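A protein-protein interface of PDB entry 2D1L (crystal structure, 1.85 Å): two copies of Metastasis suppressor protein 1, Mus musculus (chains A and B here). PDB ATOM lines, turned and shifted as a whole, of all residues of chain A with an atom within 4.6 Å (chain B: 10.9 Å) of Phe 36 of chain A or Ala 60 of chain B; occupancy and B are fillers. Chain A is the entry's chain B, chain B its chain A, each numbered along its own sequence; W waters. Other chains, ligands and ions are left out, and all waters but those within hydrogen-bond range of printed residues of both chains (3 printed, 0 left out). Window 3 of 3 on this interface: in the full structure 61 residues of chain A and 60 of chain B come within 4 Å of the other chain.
The side-chain amino group (NZ) of Lys 39 of chain A lies within hydrogen-bond range of the side-chain amide oxygen (OD1) of Asn 38 of chain A (3.3 Å). OD1 of Asp 35 of chain A lies within salt-bridge range of NZ of Lys 39 of chain A (2.5 Å).
Among the printed residues, pairs that only touch across the chains: Val 32 of chain A with Lys 63 of chain B, Val 32 of chain A with Val 64 of chain B, Val 32 of chain A with Met 67 of chain B, Trp 33 of chain A with Val 64 of chain B, Trp 33 of chain A with Met 67 of chain B, Phe 36 of chain A with Phe 57 of chain B, Phe 36 of chain A with Ala 60 of chain B, Phe 36 of chain A with Phe 61 of chain B, Phe 36 of chain A with Val 64 of chain B, Lys 39 of chain A with Ala 56 of chain B, Lys 39 of chain A with Phe 57 of chain B, Ala 40 of chain A with Phe 57 of chain B and Phe 205 of chain A with Val 64 of chain B.
Of the printed residues of chain B, Phe 36 of chain A touches Phe 57 (3.6 Å), Ala 60 (3.8 Å), Phe 61 (3.5 Å) and Val 64 (3.8 Å). Ile 37 of chain A touches none of the printed residues of chain B. Printed residues of chain B within 4 Å of Lys 39 of chain A: Ala 56 (3.8 Å) and Phe 57 (3.9 Å). Of the printed residues of chain A, Ala 60 of chain B touches Phe 36. Printed residues of chain A within 4 Å of Phe 61 of chain B: Phe 36. Of the printed residues of chain A, Val 64 of chain B touches Val 32 (3.9 Å), Trp 33 (3.6 Å), Phe 36 (3.8 Å) and Phe 205 (3.9 Å). The nearest residue of chain B that does not touch Phe 36 of chain A is Gln 62 of chain B (6.0 Å). The nearest printed residue of chain A that does not touch Ala 60 of chain B is Asp 35 of chain A (4.1 Å). The nearest printed residue of chain B that does not touch Phe 205 of chain A is Leu 82 of chain B (4.1 Å).
Of the 26 printed residues of chain B, 7 touch a printed residue of chain A. Hydrophobic or aromatic side chains of chain B that line the printed part of chain A: Phe 57, Ala 60, Phe 61, Val 64 and Met 67. Hydrophobic or aromatic side chains of chain A that line the printed part of chain B: Val 32, Trp 33, Phe 36, Ala 40 and Phe 205. Along chain A the printed residues that touch a printed residue of chain B span positions 32 to 205. Among the printed residues, 13 pairs touch across the chains.
No position is printed for both chains. Of the 13 pairs that touch across the chains among the printed residues, none has its exchanged pair printed and touching as well.
Water W1 lies within hydrogen-bond range of the side-chain amino group of Lys 63 of chain B (2.6 Å) and the side-chain carboxylate of Asp 35 of chain A (2.9 Å). Water W2 lies within hydrogen-bond range of O of Ala 53 of chain B (2.8 Å) and O of Lys 39 of chain A (2.8 Å). Water W3 lies within hydrogen-bond range of the backbone carbonyl oxygen (O) of Val 32 of chain A and the backbone carbonyl oxygen (O) of Ala 60 of chain B.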
ATOM      1  N   VAL A  32     -17.671 -28.786   7.030  1.00  0.00           N
ATOM      2  CA  VAL A  32     -16.572 -28.211   7.840  1.00  0.00           C
ATOM      3  C   VAL A  32     -15.209 -28.516   7.190  1.00  0.00           C
ATOM      4  O   VAL A  32     -14.347 -27.615   7.066  1.00  0.00           O
ATOM      5  CB  VAL A  32     -16.620 -28.758   9.264  1.00  0.00           C
ATOM      6  CG1 VAL A  32     -15.374 -28.355  10.066  1.00  0.00           C
ATOM      7  CG2 VAL A  32     -17.894 -28.256   9.933  1.00  0.00           C
ATOM      8  N   TRP A  33     -15.014 -29.764   6.777  1.00  0.00           N
ATOM      9  CA  TRP A  33     -13.767 -30.152   6.116  1.00  0.00           C
ATOM     10  C   TRP A  33     -13.631 -29.434   4.777  1.00  0.00           C
ATOM     11  O   TRP A  33     -12.540 -28.977   4.406  1.00  0.00           O
ATOM     12  CB  TRP A  33     -13.737 -31.660   5.842  1.00  0.00           C
ATOM     13  CG  TRP A  33     -13.453 -32.533   7.048  1.00  0.00           C
ATOM     14  CD1 TRP A  33     -14.296 -33.467   7.575  1.00  0.00           C
ATOM     15  CD2 TRP A  33     -12.252 -32.582   7.824  1.00  0.00           C
ATOM     16  NE1 TRP A  33     -13.706 -34.095   8.651  1.00  0.00           N
ATOM     17  CE2 TRP A  33     -12.446 -33.573   8.823  1.00  0.00           C
ATOM     18  CE3 TRP A  33     -11.034 -31.862   7.797  1.00  0.00           C
ATOM     19  CZ2 TRP A  33     -11.475 -33.872   9.778  1.00  0.00           C
ATOM     20  CZ3 TRP A  33     -10.075 -32.163   8.743  1.00  0.00           C
ATOM     21  CH2 TRP A  33     -10.292 -33.182   9.707  1.00  0.00           C
ATOM     22  N   GLU A  34     -14.738 -29.327   4.054  1.00  0.00           N
ATOM     23  CA  GLU A  34     -14.724 -28.598   2.781  1.00  0.00           C
ATOM     24  C   GLU A  34     -14.321 -27.112   2.922  1.00  0.00           C
ATOM     25  O   GLU A  34     -13.536 -26.586   2.114  1.00  0.00           O
ATOM     26  CB  GLU A  34     -16.080 -28.706   2.098  1.00  0.00           C
ATOM     27  CG  GLU A  34     -16.366 -30.095   1.607  1.00  0.00           C
ATOM     28  CD  GLU A  34     -17.837 -30.301   1.243  1.00  0.00           C
ATOM     29  OE1 GLU A  34     -18.612 -29.300   1.182  1.00  0.00           O
ATOM     30  OE2 GLU A  34     -18.211 -31.476   1.015  1.00  0.00           O
ATOM     31  N   ASP A  35     -14.890 -26.432   3.901  1.00  0.00           N
ATOM     32  CA  ASP A  35     -14.563 -25.024   4.114  1.00  0.00           C
ATOM     33  C   ASP A  35     -13.106 -24.853   4.482  1.00  0.00           C
ATOM     34  O   ASP A  35     -12.459 -23.934   4.010  1.00  0.00           O
ATOM     35  CB  ASP A  35     -15.448 -24.385   5.172  1.00  0.00           C
ATOM     36  CG  ASP A  35     -15.273 -22.854   5.236  1.00  0.00           C
ATOM     37  OD1 ASP A  35     -15.194 -22.214   4.180  1.00  0.00           O
ATOM     38  OD2 ASP A  35     -15.198 -22.310   6.347  1.00  0.00           O
ATOM     39  N   PHE A  36     -12.595 -25.760   5.303  1.00  0.00           N
ATOM     40  CA  PHE A  36     -11.162 -25.803   5.622  1.00  0.00           C
ATOM     41  C   PHE A  36     -10.297 -25.931   4.347  1.00  0.00           C
ATOM     42  O   PHE A  36      -9.349 -25.171   4.139  1.00  0.00           O
ATOM     43  CB  PHE A  36     -10.863 -26.957   6.594  1.00  0.00           C
ATOM     44  CG  PHE A  36      -9.409 -27.050   6.981  1.00  0.00           C
ATOM     45  CD1 PHE A  36      -8.927 -26.266   8.013  1.00  0.00           C
ATOM     46  CD2 PHE A  36      -8.509 -27.836   6.250  1.00  0.00           C
ATOM     47  CE1 PHE A  36      -7.609 -26.301   8.372  1.00  0.00           C
ATOM     48  CE2 PHE A  36      -7.173 -27.884   6.582  1.00  0.00           C
ATOM     49  CZ  PHE A  36      -6.710 -27.111   7.646  1.00  0.00           C
ATOM     50  N   ILE A  37     -10.632 -26.867   3.479  1.00  0.00           N
ATOM     51  CA  ILE A  37      -9.845 -27.055   2.255  1.00  0.00           C
ATOM     52  C   ILE A  37      -9.928 -25.775   1.421  1.00  0.00           C
ATOM     53  O   ILE A  37      -8.932 -25.336   0.841  1.00  0.00           O
ATOM     54  CB  ILE A  37     -10.378 -28.248   1.441  1.00  0.00           C
ATOM     55  CG1 ILE A  37     -10.103 -29.581   2.176  1.00  0.00           C
ATOM     56  CG2 ILE A  37      -9.758 -28.272   0.047  1.00  0.00           C
ATOM     57  CD1 ILE A  37     -10.816 -30.770   1.462  1.00  0.00           C
ATOM     58  N   ASN A  38     -11.112 -25.177   1.380  1.00  0.00           N
ATOM     59  CA  ASN A  38     -11.322 -23.945   0.594  1.00  0.00           C
ATOM     60  C   ASN A  38     -10.453 -22.773   1.137  1.00  0.00           C
ATOM     61  O   ASN A  38      -9.778 -22.070   0.377  1.00  0.00           O
ATOM     62  CB  ASN A  38     -12.789 -23.500   0.591  1.00  0.00           C
ATOM     63  CG  ASN A  38     -12.997 -22.215  -0.215  1.00  0.00           C
ATOM     64  OD1 ASN A  38     -13.427 -21.188   0.312  1.00  0.00           O
ATOM     65  ND2 ASN A  38     -12.659 -22.267  -1.500  1.00  0.00           N
ATOM     66  N   LYS A  39     -10.507 -22.552   2.436  1.00  0.00           N
ATOM     67  CA  LYS A  39      -9.758 -21.444   3.037  1.00  0.00           C
ATOM     68  C   LYS A  39      -8.251 -21.678   3.020  1.00  0.00           C
ATOM     69  O   LYS A  39      -7.458 -20.714   2.878  1.00  0.00           O
ATOM     70  CB  LYS A  39     -10.235 -21.161   4.464  1.00  0.00           C
ATOM     71  CG  LYS A  39     -11.642 -20.548   4.559  1.00  0.00           C
ATOM     72  CD  LYS A  39     -12.040 -19.739   3.328  1.00  0.00           C
ATOM     73  CE  LYS A  39     -13.431 -19.098   3.486  1.00  0.00           C
ATOM     74  NZ  LYS A  39     -14.562 -20.031   3.213  1.00  0.00           N
ATOM     75  N   ALA A  40      -7.846 -22.941   3.170  1.00  0.00           N
ATOM     76  CA  ALA A  40      -6.426 -23.279   3.114  1.00  0.00           C
ATOM     77  C   ALA A  40      -5.945 -22.984   1.677  1.00  0.00           C
ATOM     78  O   ALA A  40      -4.856 -22.453   1.471  1.00  0.00           O
ATOM     79  CB  ALA A  40      -6.216 -24.771   3.426  1.00  0.00           C
ATOM     80  N   LEU A 107      -0.789 -31.023   2.584  1.00  0.00           N
ATOM     81  CA  LEU A 107      -2.076 -30.896   3.232  1.00  0.00           C
ATOM     82  C   LEU A 107      -3.285 -30.726   2.316  1.00  0.00           C
ATOM     83  O   LEU A 107      -4.215 -31.503   2.394  1.00  0.00           O
ATOM     84  CB  LEU A 107      -2.027 -29.761   4.264  1.00  0.00           C
ATOM     85  CG  LEU A 107      -3.306 -29.429   5.038  1.00  0.00           C
ATOM     86  CD1 LEU A 107      -3.847 -30.644   5.833  1.00  0.00           C
ATOM     87  CD2 LEU A 107      -3.017 -28.262   5.929  1.00  0.00           C
ATOM     88  N   LEU A 111      -5.692 -33.844   1.506  1.00  0.00           N
ATOM     89  CA  LEU A 111      -6.947 -33.815   2.285  1.00  0.00           C
ATOM     90  C   LEU A 111      -8.139 -33.857   1.350  1.00  0.00           C
ATOM     91  O   LEU A 111      -9.137 -34.556   1.604  1.00  0.00           O
ATOM     92  CB  LEU A 111      -7.011 -32.590   3.198  1.00  0.00           C
ATOM     93  CG  LEU A 111      -8.186 -32.447   4.173  1.00  0.00           C
ATOM     94  CD1 LEU A 111      -8.342 -33.668   5.034  1.00  0.00           C
ATOM     95  CD2 LEU A 111      -7.982 -31.183   5.032  1.00  0.00           C
ATOM     96  N   PHE A 205      -5.419 -36.418   9.349  1.00  0.00           N
ATOM     97  CA  PHE A 205      -5.318 -34.958   9.141  1.00  0.00           C
ATOM     98  C   PHE A 205      -4.058 -34.438   9.827  1.00  0.00           C
ATOM     99  O   PHE A 205      -3.335 -33.600   9.291  1.00  0.00           O
ATOM    100  CB  PHE A 205      -6.599 -34.272   9.650  1.00  0.00           C
ATOM    101  CG  PHE A 205      -6.506 -32.763   9.801  1.00  0.00           C
ATOM    102  CD1 PHE A 205      -6.370 -31.951   8.692  1.00  0.00           C
ATOM    103  CD2 PHE A 205      -6.598 -32.162  11.057  1.00  0.00           C
ATOM    104  CE1 PHE A 205      -6.333 -30.532   8.820  1.00  0.00           C
ATOM    105  CE2 PHE A 205      -6.545 -30.761  11.201  1.00  0.00           C
ATOM    106  CZ  PHE A 205      -6.399 -29.954  10.082  1.00  0.00           C
ATOM    107  N   VAL B  52      -5.353 -11.280   5.938  1.00  0.00           N
ATOM    108  CA  VAL B  52      -6.802 -11.546   5.894  1.00  0.00           C
ATOM    109  C   VAL B  52      -7.056 -13.023   5.533  1.00  0.00           C
ATOM    110  O   VAL B  52      -7.913 -13.691   6.131  1.00  0.00           O
ATOM    111  CB  VAL B  52      -7.517 -10.621   4.895  1.00  0.00           C
ATOM    112  CG1 VAL B  52      -8.977 -11.037   4.694  1.00  0.00           C
ATOM    113  CG2 VAL B  52      -7.385  -9.134   5.317  1.00  0.00           C
ATOM    114  N   ALA B  53      -6.339 -13.536   4.545  1.00  0.00           N
ATOM    115  CA  ALA B  53      -6.536 -14.940   4.161  1.00  0.00           C
ATOM    116  C   ALA B  53      -6.080 -15.883   5.304  1.00  0.00           C
ATOM    117  O   ALA B  53      -6.712 -16.923   5.558  1.00  0.00           O
ATOM    118  CB  ALA B  53      -5.808 -15.265   2.829  1.00  0.00           C
ATOM    119  N   ALA B  54      -5.044 -15.488   6.029  1.00  0.00           N
ATOM    120  CA  ALA B  54      -4.572 -16.312   7.173  1.00  0.00           C
ATOM    121  C   ALA B  54      -5.642 -16.334   8.280  1.00  0.00           C
ATOM    122  O   ALA B  54      -5.881 -17.378   8.925  1.00  0.00           O
ATOM    123  CB  ALA B  54      -3.224 -15.774   7.711  1.00  0.00           C
ATOM    124  N   ALA B  55      -6.286 -15.190   8.526  1.00  0.00           N
ATOM    125  CA  ALA B  55      -7.317 -15.167   9.590  1.00  0.00           C
ATOM    126  C   ALA B  55      -8.503 -16.035   9.185  1.00  0.00           C
ATOM    127  O   ALA B  55      -9.095 -16.687  10.024  1.00  0.00           O
ATOM    128  CB  ALA B  55      -7.797 -13.776   9.862  1.00  0.00           C
ATOM    129  N   ALA B  56      -8.856 -16.040   7.901  1.00  0.00           N
ATOM    130  CA  ALA B  56     -10.001 -16.853   7.463  1.00  0.00           C
ATOM    131  C   ALA B  56      -9.660 -18.344   7.538  1.00  0.00           C
ATOM    132  O   ALA B  56     -10.478 -19.176   7.911  1.00  0.00           O
ATOM    133  CB  ALA B  56     -10.458 -16.439   6.053  1.00  0.00           C
ATOM    134  N   PHE B  57      -8.427 -18.671   7.192  1.00  0.00           N
ATOM    135  CA  PHE B  57      -7.931 -20.026   7.357  1.00  0.00           C
ATOM    136  C   PHE B  57      -7.970 -20.457   8.833  1.00  0.00           C
ATOM    137  O   PHE B  57      -8.452 -21.557   9.157  1.00  0.00           O
ATOM    138  CB  PHE B  57      -6.513 -20.136   6.802  1.00  0.00           C
ATOM    139  CG  PHE B  57      -5.821 -21.432   7.162  1.00  0.00           C
ATOM    140  CD1 PHE B  57      -6.172 -22.622   6.527  1.00  0.00           C
ATOM    141  CD2 PHE B  57      -4.852 -21.460   8.134  1.00  0.00           C
ATOM    142  CE1 PHE B  57      -5.530 -23.815   6.844  1.00  0.00           C
ATOM    143  CE2 PHE B  57      -4.197 -22.668   8.473  1.00  0.00           C
ATOM    144  CZ  PHE B  57      -4.533 -23.833   7.813  1.00  0.00           C
ATOM    145  N   LEU B  58      -7.471 -19.616   9.739  1.00  0.00           N
ATOM    146  CA  LEU B  58      -7.517 -19.978  11.134  1.00  0.00           C
ATOM    147  C   LEU B  58      -8.951 -20.149  11.671  1.00  0.00           C
ATOM    148  O   LEU B  58      -9.196 -21.036  12.493  1.00  0.00           O
ATOM    149  CB  LEU B  58      -6.690 -18.999  12.009  1.00  0.00           C
ATOM    150  CG  LEU B  58      -5.182 -19.064  11.693  1.00  0.00           C
ATOM    151  CD1 LEU B  58      -4.436 -17.955  12.469  1.00  0.00           C
ATOM    152  CD2 LEU B  58      -4.572 -20.470  11.950  1.00  0.00           C
ATOM    153  N   ASP B  59      -9.895 -19.319  11.212  1.00  0.00           N
ATOM    154  CA  ASP B  59     -11.301 -19.521  11.565  1.00  0.00           C
ATOM    155  C   ASP B  59     -11.762 -20.931  11.161  1.00  0.00           C
ATOM    156  O   ASP B  59     -12.428 -21.633  11.942  1.00  0.00           O
ATOM    157  CB  ASP B  59     -12.219 -18.477  10.922  1.00  0.00           C
ATOM    158  CG  ASP B  59     -11.995 -17.061  11.461  1.00  0.00           C
ATOM    159  OD1 ASP B  59     -11.350 -16.869  12.525  1.00  0.00           O
ATOM    160  OD2 ASP B  59     -12.500 -16.134  10.805  1.00  0.00           O
ATOM    161  N   ALA B  60     -11.403 -21.355   9.947  1.00  0.00           N
ATOM    162  CA  ALA B  60     -11.800 -22.690   9.468  1.00  0.00           C
ATOM    163  C   ALA B  60     -11.107 -23.773  10.254  1.00  0.00           C
ATOM    164  O   ALA B  60     -11.690 -24.831  10.537  1.00  0.00           O
ATOM    165  CB  ALA B  60     -11.503 -22.866   7.950  1.00  0.00           C
ATOM    166  N   PHE B  61      -9.839 -23.524  10.593  1.00  0.00           N
ATOM    167  CA  PHE B  61      -9.024 -24.510  11.309  1.00  0.00           C
ATOM    168  C   PHE B  61      -9.662 -24.725  12.685  1.00  0.00           C
ATOM    169  O   PHE B  61      -9.803 -25.846  13.142  1.00  0.00           O
ATOM    170  CB  PHE B  61      -7.615 -23.934  11.489  1.00  0.00           C
ATOM    171  CG  PHE B  61      -6.625 -24.912  12.091  1.00  0.00           C
ATOM    172  CD1 PHE B  61      -5.739 -25.593  11.295  1.00  0.00           C
ATOM    173  CD2 PHE B  61      -6.595 -25.134  13.467  1.00  0.00           C
ATOM    174  CE1 PHE B  61      -4.822 -26.509  11.857  1.00  0.00           C
ATOM    175  CE2 PHE B  61      -5.684 -26.032  14.032  1.00  0.00           C
ATOM    176  CZ  PHE B  61      -4.808 -26.710  13.237  1.00  0.00           C
ATOM    177  N   GLN B  62     -10.096 -23.643  13.314  1.00  0.00           N
ATOM    178  CA  GLN B  62     -10.749 -23.738  14.626  1.00  0.00           C
ATOM    179  C   GLN B  62     -12.078 -24.520  14.592  1.00  0.00           C
ATOM    180  O   GLN B  62     -12.393 -25.290  15.514  1.00  0.00           O
ATOM    181  CB  GLN B  62     -10.940 -22.350  15.252  1.00  0.00           C
ATOM    182  CG  GLN B  62     -11.518 -22.456  16.660  1.00  0.00           C
ATOM    183  CD  GLN B  62     -10.597 -23.161  17.619  1.00  0.00           C
ATOM    184  OE1 GLN B  62      -9.420 -22.797  17.766  1.00  0.00           O
ATOM    185  NE2 GLN B  62     -11.122 -24.172  18.292  1.00  0.00           N
ATOM    186  N   LYS B  63     -12.837 -24.370  13.514  1.00  0.00           N
ATOM    187  CA  LYS B  63     -14.044 -25.192  13.365  1.00  0.00           C
ATOM    188  C   LYS B  63     -13.756 -26.687  13.257  1.00  0.00           C
ATOM    189  O   LYS B  63     -14.563 -27.518  13.714  1.00  0.00           O
ATOM    190  CB  LYS B  63     -14.842 -24.714  12.159  1.00  0.00           C
ATOM    191  CG  LYS B  63     -15.419 -23.326  12.457  1.00  0.00           C
ATOM    192  CD  LYS B  63     -15.963 -22.652  11.244  1.00  0.00           C
ATOM    193  CE  LYS B  63     -16.030 -21.140  11.481  1.00  0.00           C
ATOM    194  NZ  LYS B  63     -16.590 -20.394  10.311  1.00  0.00           N
ATOM    195  N   VAL B  64     -12.642 -27.025  12.600  1.00  0.00           N
ATOM    196  CA  VAL B  64     -12.166 -28.420  12.560  1.00  0.00           C
ATOM    197  C   VAL B  64     -11.814 -28.911  13.976  1.00  0.00           C
ATOM    198  O   VAL B  64     -12.256 -29.987  14.383  1.00  0.00           O
ATOM    199  CB  VAL B  64     -10.973 -28.558  11.572  1.00  0.00           C
ATOM    200  CG1 VAL B  64     -10.323 -29.996  11.658  1.00  0.00           C
ATOM    201  CG2 VAL B  64     -11.461 -28.194  10.145  1.00  0.00           C
ATOM    202  N   ALA B  65     -11.055 -28.104  14.719  1.00  0.00           N
ATOM    203  CA  ALA B  65     -10.667 -28.401  16.090  1.00  0.00           C
ATOM    204  C   ALA B  65     -11.917 -28.607  16.965  1.00  0.00           C
ATOM    205  O   ALA B  65     -11.985 -29.555  17.757  1.00  0.00           O
ATOM    206  CB  ALA B  65      -9.802 -27.233  16.656  1.00  0.00           C
ATOM    207  N   ASP B  66     -12.901 -27.718  16.807  1.00  0.00           N
ATOM    208  CA  ASP B  66     -14.185 -27.790  17.566  1.00  0.00           C
ATOM    209  C   ASP B  66     -14.880 -29.115  17.282  1.00  0.00           C
ATOM    210  O   ASP B  66     -15.432 -29.762  18.181  1.00  0.00           O
ATOM    211  CB  ASP B  66     -15.148 -26.690  17.103  1.00  0.00           C
ATOM    212  CG  ASP B  66     -14.764 -25.290  17.609  1.00  0.00           C
ATOM    213  OD1 ASP B  66     -13.924 -25.168  18.526  1.00  0.00           O
ATOM    214  OD2 ASP B  66     -15.319 -24.293  17.068  1.00  0.00           O
ATOM    215  N   MET B  67     -14.921 -29.480  16.012  1.00  0.00           N
ATOM    216  CA  MET B  67     -15.543 -30.738  15.613  1.00  0.00           C
ATOM    217  C   MET B  67     -14.914 -31.931  16.343  1.00  0.00           C
ATOM    218  O   MET B  67     -15.629 -32.766  16.901  1.00  0.00           O
ATOM    219  CB  MET B  67     -15.421 -30.897  14.092  1.00  0.00           C
ATOM    220  CG  MET B  67     -16.182 -32.037  13.494  1.00  0.00           C
ATOM    221  SD  MET B  67     -16.371 -31.662  11.588  1.00  0.00           S
ATOM    222  CE  MET B  67     -14.420 -31.736  11.056  1.00  0.00           C
ATOM    223  N   ALA B  68     -13.581 -32.020  16.352  1.00  0.00           N
ATOM    224  CA  ALA B  68     -12.906 -33.103  17.093  1.00  0.00           C
ATOM    225  C   ALA B  68     -13.152 -33.034  18.584  1.00  0.00           C
ATOM    226  O   ALA B  68     -13.374 -34.055  19.245  1.00  0.00           O
ATOM    227  CB  ALA B  68     -11.377 -33.076  16.841  1.00  0.00           C
ATOM    228  N   GLY B  79      -8.811 -32.746  19.585  1.00  0.00           N
ATOM    229  CA  GLY B  79      -9.474 -31.443  19.382  1.00  0.00           C
ATOM    230  C   GLY B  79      -8.883 -30.362  20.266  1.00  0.00           C
ATOM    231  O   GLY B  79      -8.595 -29.259  19.809  1.00  0.00           O
ATOM    232  N   LEU B  82      -5.494 -29.365  18.941  1.00  0.00           N
ATOM    233  CA  LEU B  82      -5.635 -28.599  17.698  1.00  0.00           C
ATOM    234  C   LEU B  82      -6.017 -27.143  18.020  1.00  0.00           C
ATOM    235  O   LEU B  82      -5.577 -26.198  17.341  1.00  0.00           O
ATOM    236  CB  LEU B  82      -6.702 -29.229  16.809  1.00  0.00           C
ATOM    237  CG  LEU B  82      -6.247 -30.447  15.985  1.00  0.00           C
ATOM    238  CD1 LEU B  82      -7.429 -31.073  15.211  1.00  0.00           C
ATOM    239  CD2 LEU B  82      -5.081 -30.075  15.016  1.00  0.00           C
ATOM    240  N   THR B  83      -6.864 -26.972  19.032  1.00  0.00           N
ATOM    241  CA  THR B  83      -7.231 -25.620  19.488  1.00  0.00           C
ATOM    242  C   THR B  83      -5.984 -24.883  20.006  1.00  0.00           C
ATOM    243  O   THR B  83      -5.771 -23.716  19.705  1.00  0.00           O
ATOM    244  CB  THR B  83      -8.366 -25.689  20.541  1.00  0.00           C
ATOM    245  OG1 THR B  83      -9.541 -26.183  19.879  1.00  0.00           O
ATOM    246  CG2 THR B  83      -8.681 -24.265  21.111  1.00  0.00           C
ATOM    247  N   MET B  85      -2.968 -25.387  18.959  1.00  0.00           N
ATOM    248  CA  MET B  85      -2.234 -25.007  17.749  1.00  0.00           C
ATOM    249  C   MET B  85      -2.822 -23.752  17.101  1.00  0.00           C
ATOM    250  O   MET B  85      -2.092 -22.847  16.713  1.00  0.00           O
ATOM    251  CB  MET B  85      -2.203 -26.155  16.711  1.00  0.00           C
ATOM    252  CG  MET B  85      -1.180 -25.928  15.584  1.00  0.00           C
ATOM    253  SD  MET B  85       0.708 -25.712  16.180  1.00  0.00           S
ATOM    254  CE  MET B  85       1.272 -27.542  16.474  1.00  0.00           C
ATOM    255  N   CYS B  86      -4.134 -23.721  16.977  1.00  0.00           N
ATOM    256  CA  CYS B  86      -4.820 -22.621  16.315  1.00  0.00           C
ATOM    257  C   CYS B  86      -4.587 -21.319  17.101  1.00  0.00           C
ATOM    258  O   CYS B  86      -4.166 -20.294  16.520  1.00  0.00           O
ATOM    259  CB  CYS B  86      -6.307 -22.920  16.211  1.00  0.00           C
ATOM    260  SG  CYS B  86      -7.112 -21.793  15.060  1.00  0.00           S
ATOM    261  N   MET B  87      -4.744 -21.360  18.417  1.00  0.00           N
ATOM    262  CA  MET B  87      -4.528 -20.126  19.183  1.00  0.00           C
ATOM    263  C   MET B  87      -3.089 -19.604  19.073  1.00  0.00           C
ATOM    264  O   MET B  87      -2.854 -18.392  19.058  1.00  0.00           O
ATOM    265  CB  MET B  87      -4.879 -20.356  20.654  1.00  0.00           C
ATOM    266  CG  MET B  87      -6.394 -20.563  20.919  1.00  0.00           C
ATOM    267  SD  MET B  87      -6.779 -20.839  22.853  1.00  0.00           S
ATOM    268  CE  MET B  87      -5.841 -22.455  23.181  1.00  0.00           C
ATOM    269  N   HIS B  89      -1.174 -19.969  16.532  1.00  0.00           N
ATOM    270  CA  HIS B  89      -1.119 -19.296  15.209  1.00  0.00           C
ATOM    271  C   HIS B  89      -1.770 -17.935  15.183  1.00  0.00           C
ATOM    272  O   HIS B  89      -1.362 -17.068  14.408  1.00  0.00           O
ATOM    273  CB  HIS B  89      -1.623 -20.209  14.084  1.00  0.00           C
ATOM    274  CG  HIS B  89      -0.617 -21.223  13.645  1.00  0.00           C
ATOM    275  ND1 HIS B  89      -0.452 -22.436  14.272  1.00  0.00           N
ATOM    276  CD2 HIS B  89       0.284 -21.193  12.642  1.00  0.00           C
ATOM    277  CE1 HIS B  89       0.498 -23.120  13.661  1.00  0.00           C
ATOM    278  NE2 HIS B  89       0.957 -22.387  12.662  1.00  0.00           N
ATOM    279  N   ARG B  90      -2.771 -17.689  16.029  1.00  0.00           N
ATOM    280  CA  ARG B  90      -3.316 -16.338  16.107  1.00  0.00           C
ATOM    281  C   ARG B  90      -2.253 -15.334  16.547  1.00  0.00           C
ATOM    282  O   ARG B  90      -2.279 -14.190  16.119  1.00  0.00           O
ATOM    283  CB  ARG B  90      -4.473 -16.254  17.092  1.00  0.00           C
ATOM    284  CG  ARG B  90      -5.639 -17.048  16.698  1.00  0.00           C
ATOM    285  CD  ARG B  90      -6.260 -16.501  15.451  1.00  0.00           C
ATOM    286  NE  ARG B  90      -7.534 -17.168  15.254  1.00  0.00           N
ATOM    287  CZ  ARG B  90      -8.372 -16.876  14.277  1.00  0.00           C
ATOM    288  NH1 ARG B  90      -8.049 -15.953  13.394  1.00  0.00           N
ATOM    289  NH2 ARG B  90      -9.497 -17.549  14.173  1.00  0.00           N
ATOM    290  N   GLU B  93      -0.160 -14.606  13.418  1.00  0.00           N
ATOM    291  CA  GLU B  93      -0.948 -13.729  12.552  1.00  0.00           C
ATOM    292  C   GLU B  93      -0.888 -12.264  13.041  1.00  0.00           C
ATOM    293  O   GLU B  93      -0.731 -11.306  12.240  1.00  0.00           O
ATOM    294  CB  GLU B  93      -2.399 -14.227  12.489  1.00  0.00           C
ATOM    295  CG  GLU B  93      -3.365 -13.320  11.714  1.00  0.00           C
ATOM    296  CD  GLU B  93      -4.812 -13.390  12.230  1.00  0.00           C
ATOM    297  OE1 GLU B  93      -5.465 -12.331  12.273  1.00  0.00           O
ATOM    298  OE2 GLU B  93      -5.310 -14.490  12.581  1.00  0.00           O
HETATM  299  O   HOH W   1     -14.640 -20.762   8.681  1.00  0.00           O
HETATM  300  O   HOH W   2      -8.200 -18.144   3.590  1.00  0.00           O
HETATM  301  O   HOH W   3     -13.934 -25.272   8.635  1.00  0.00           O
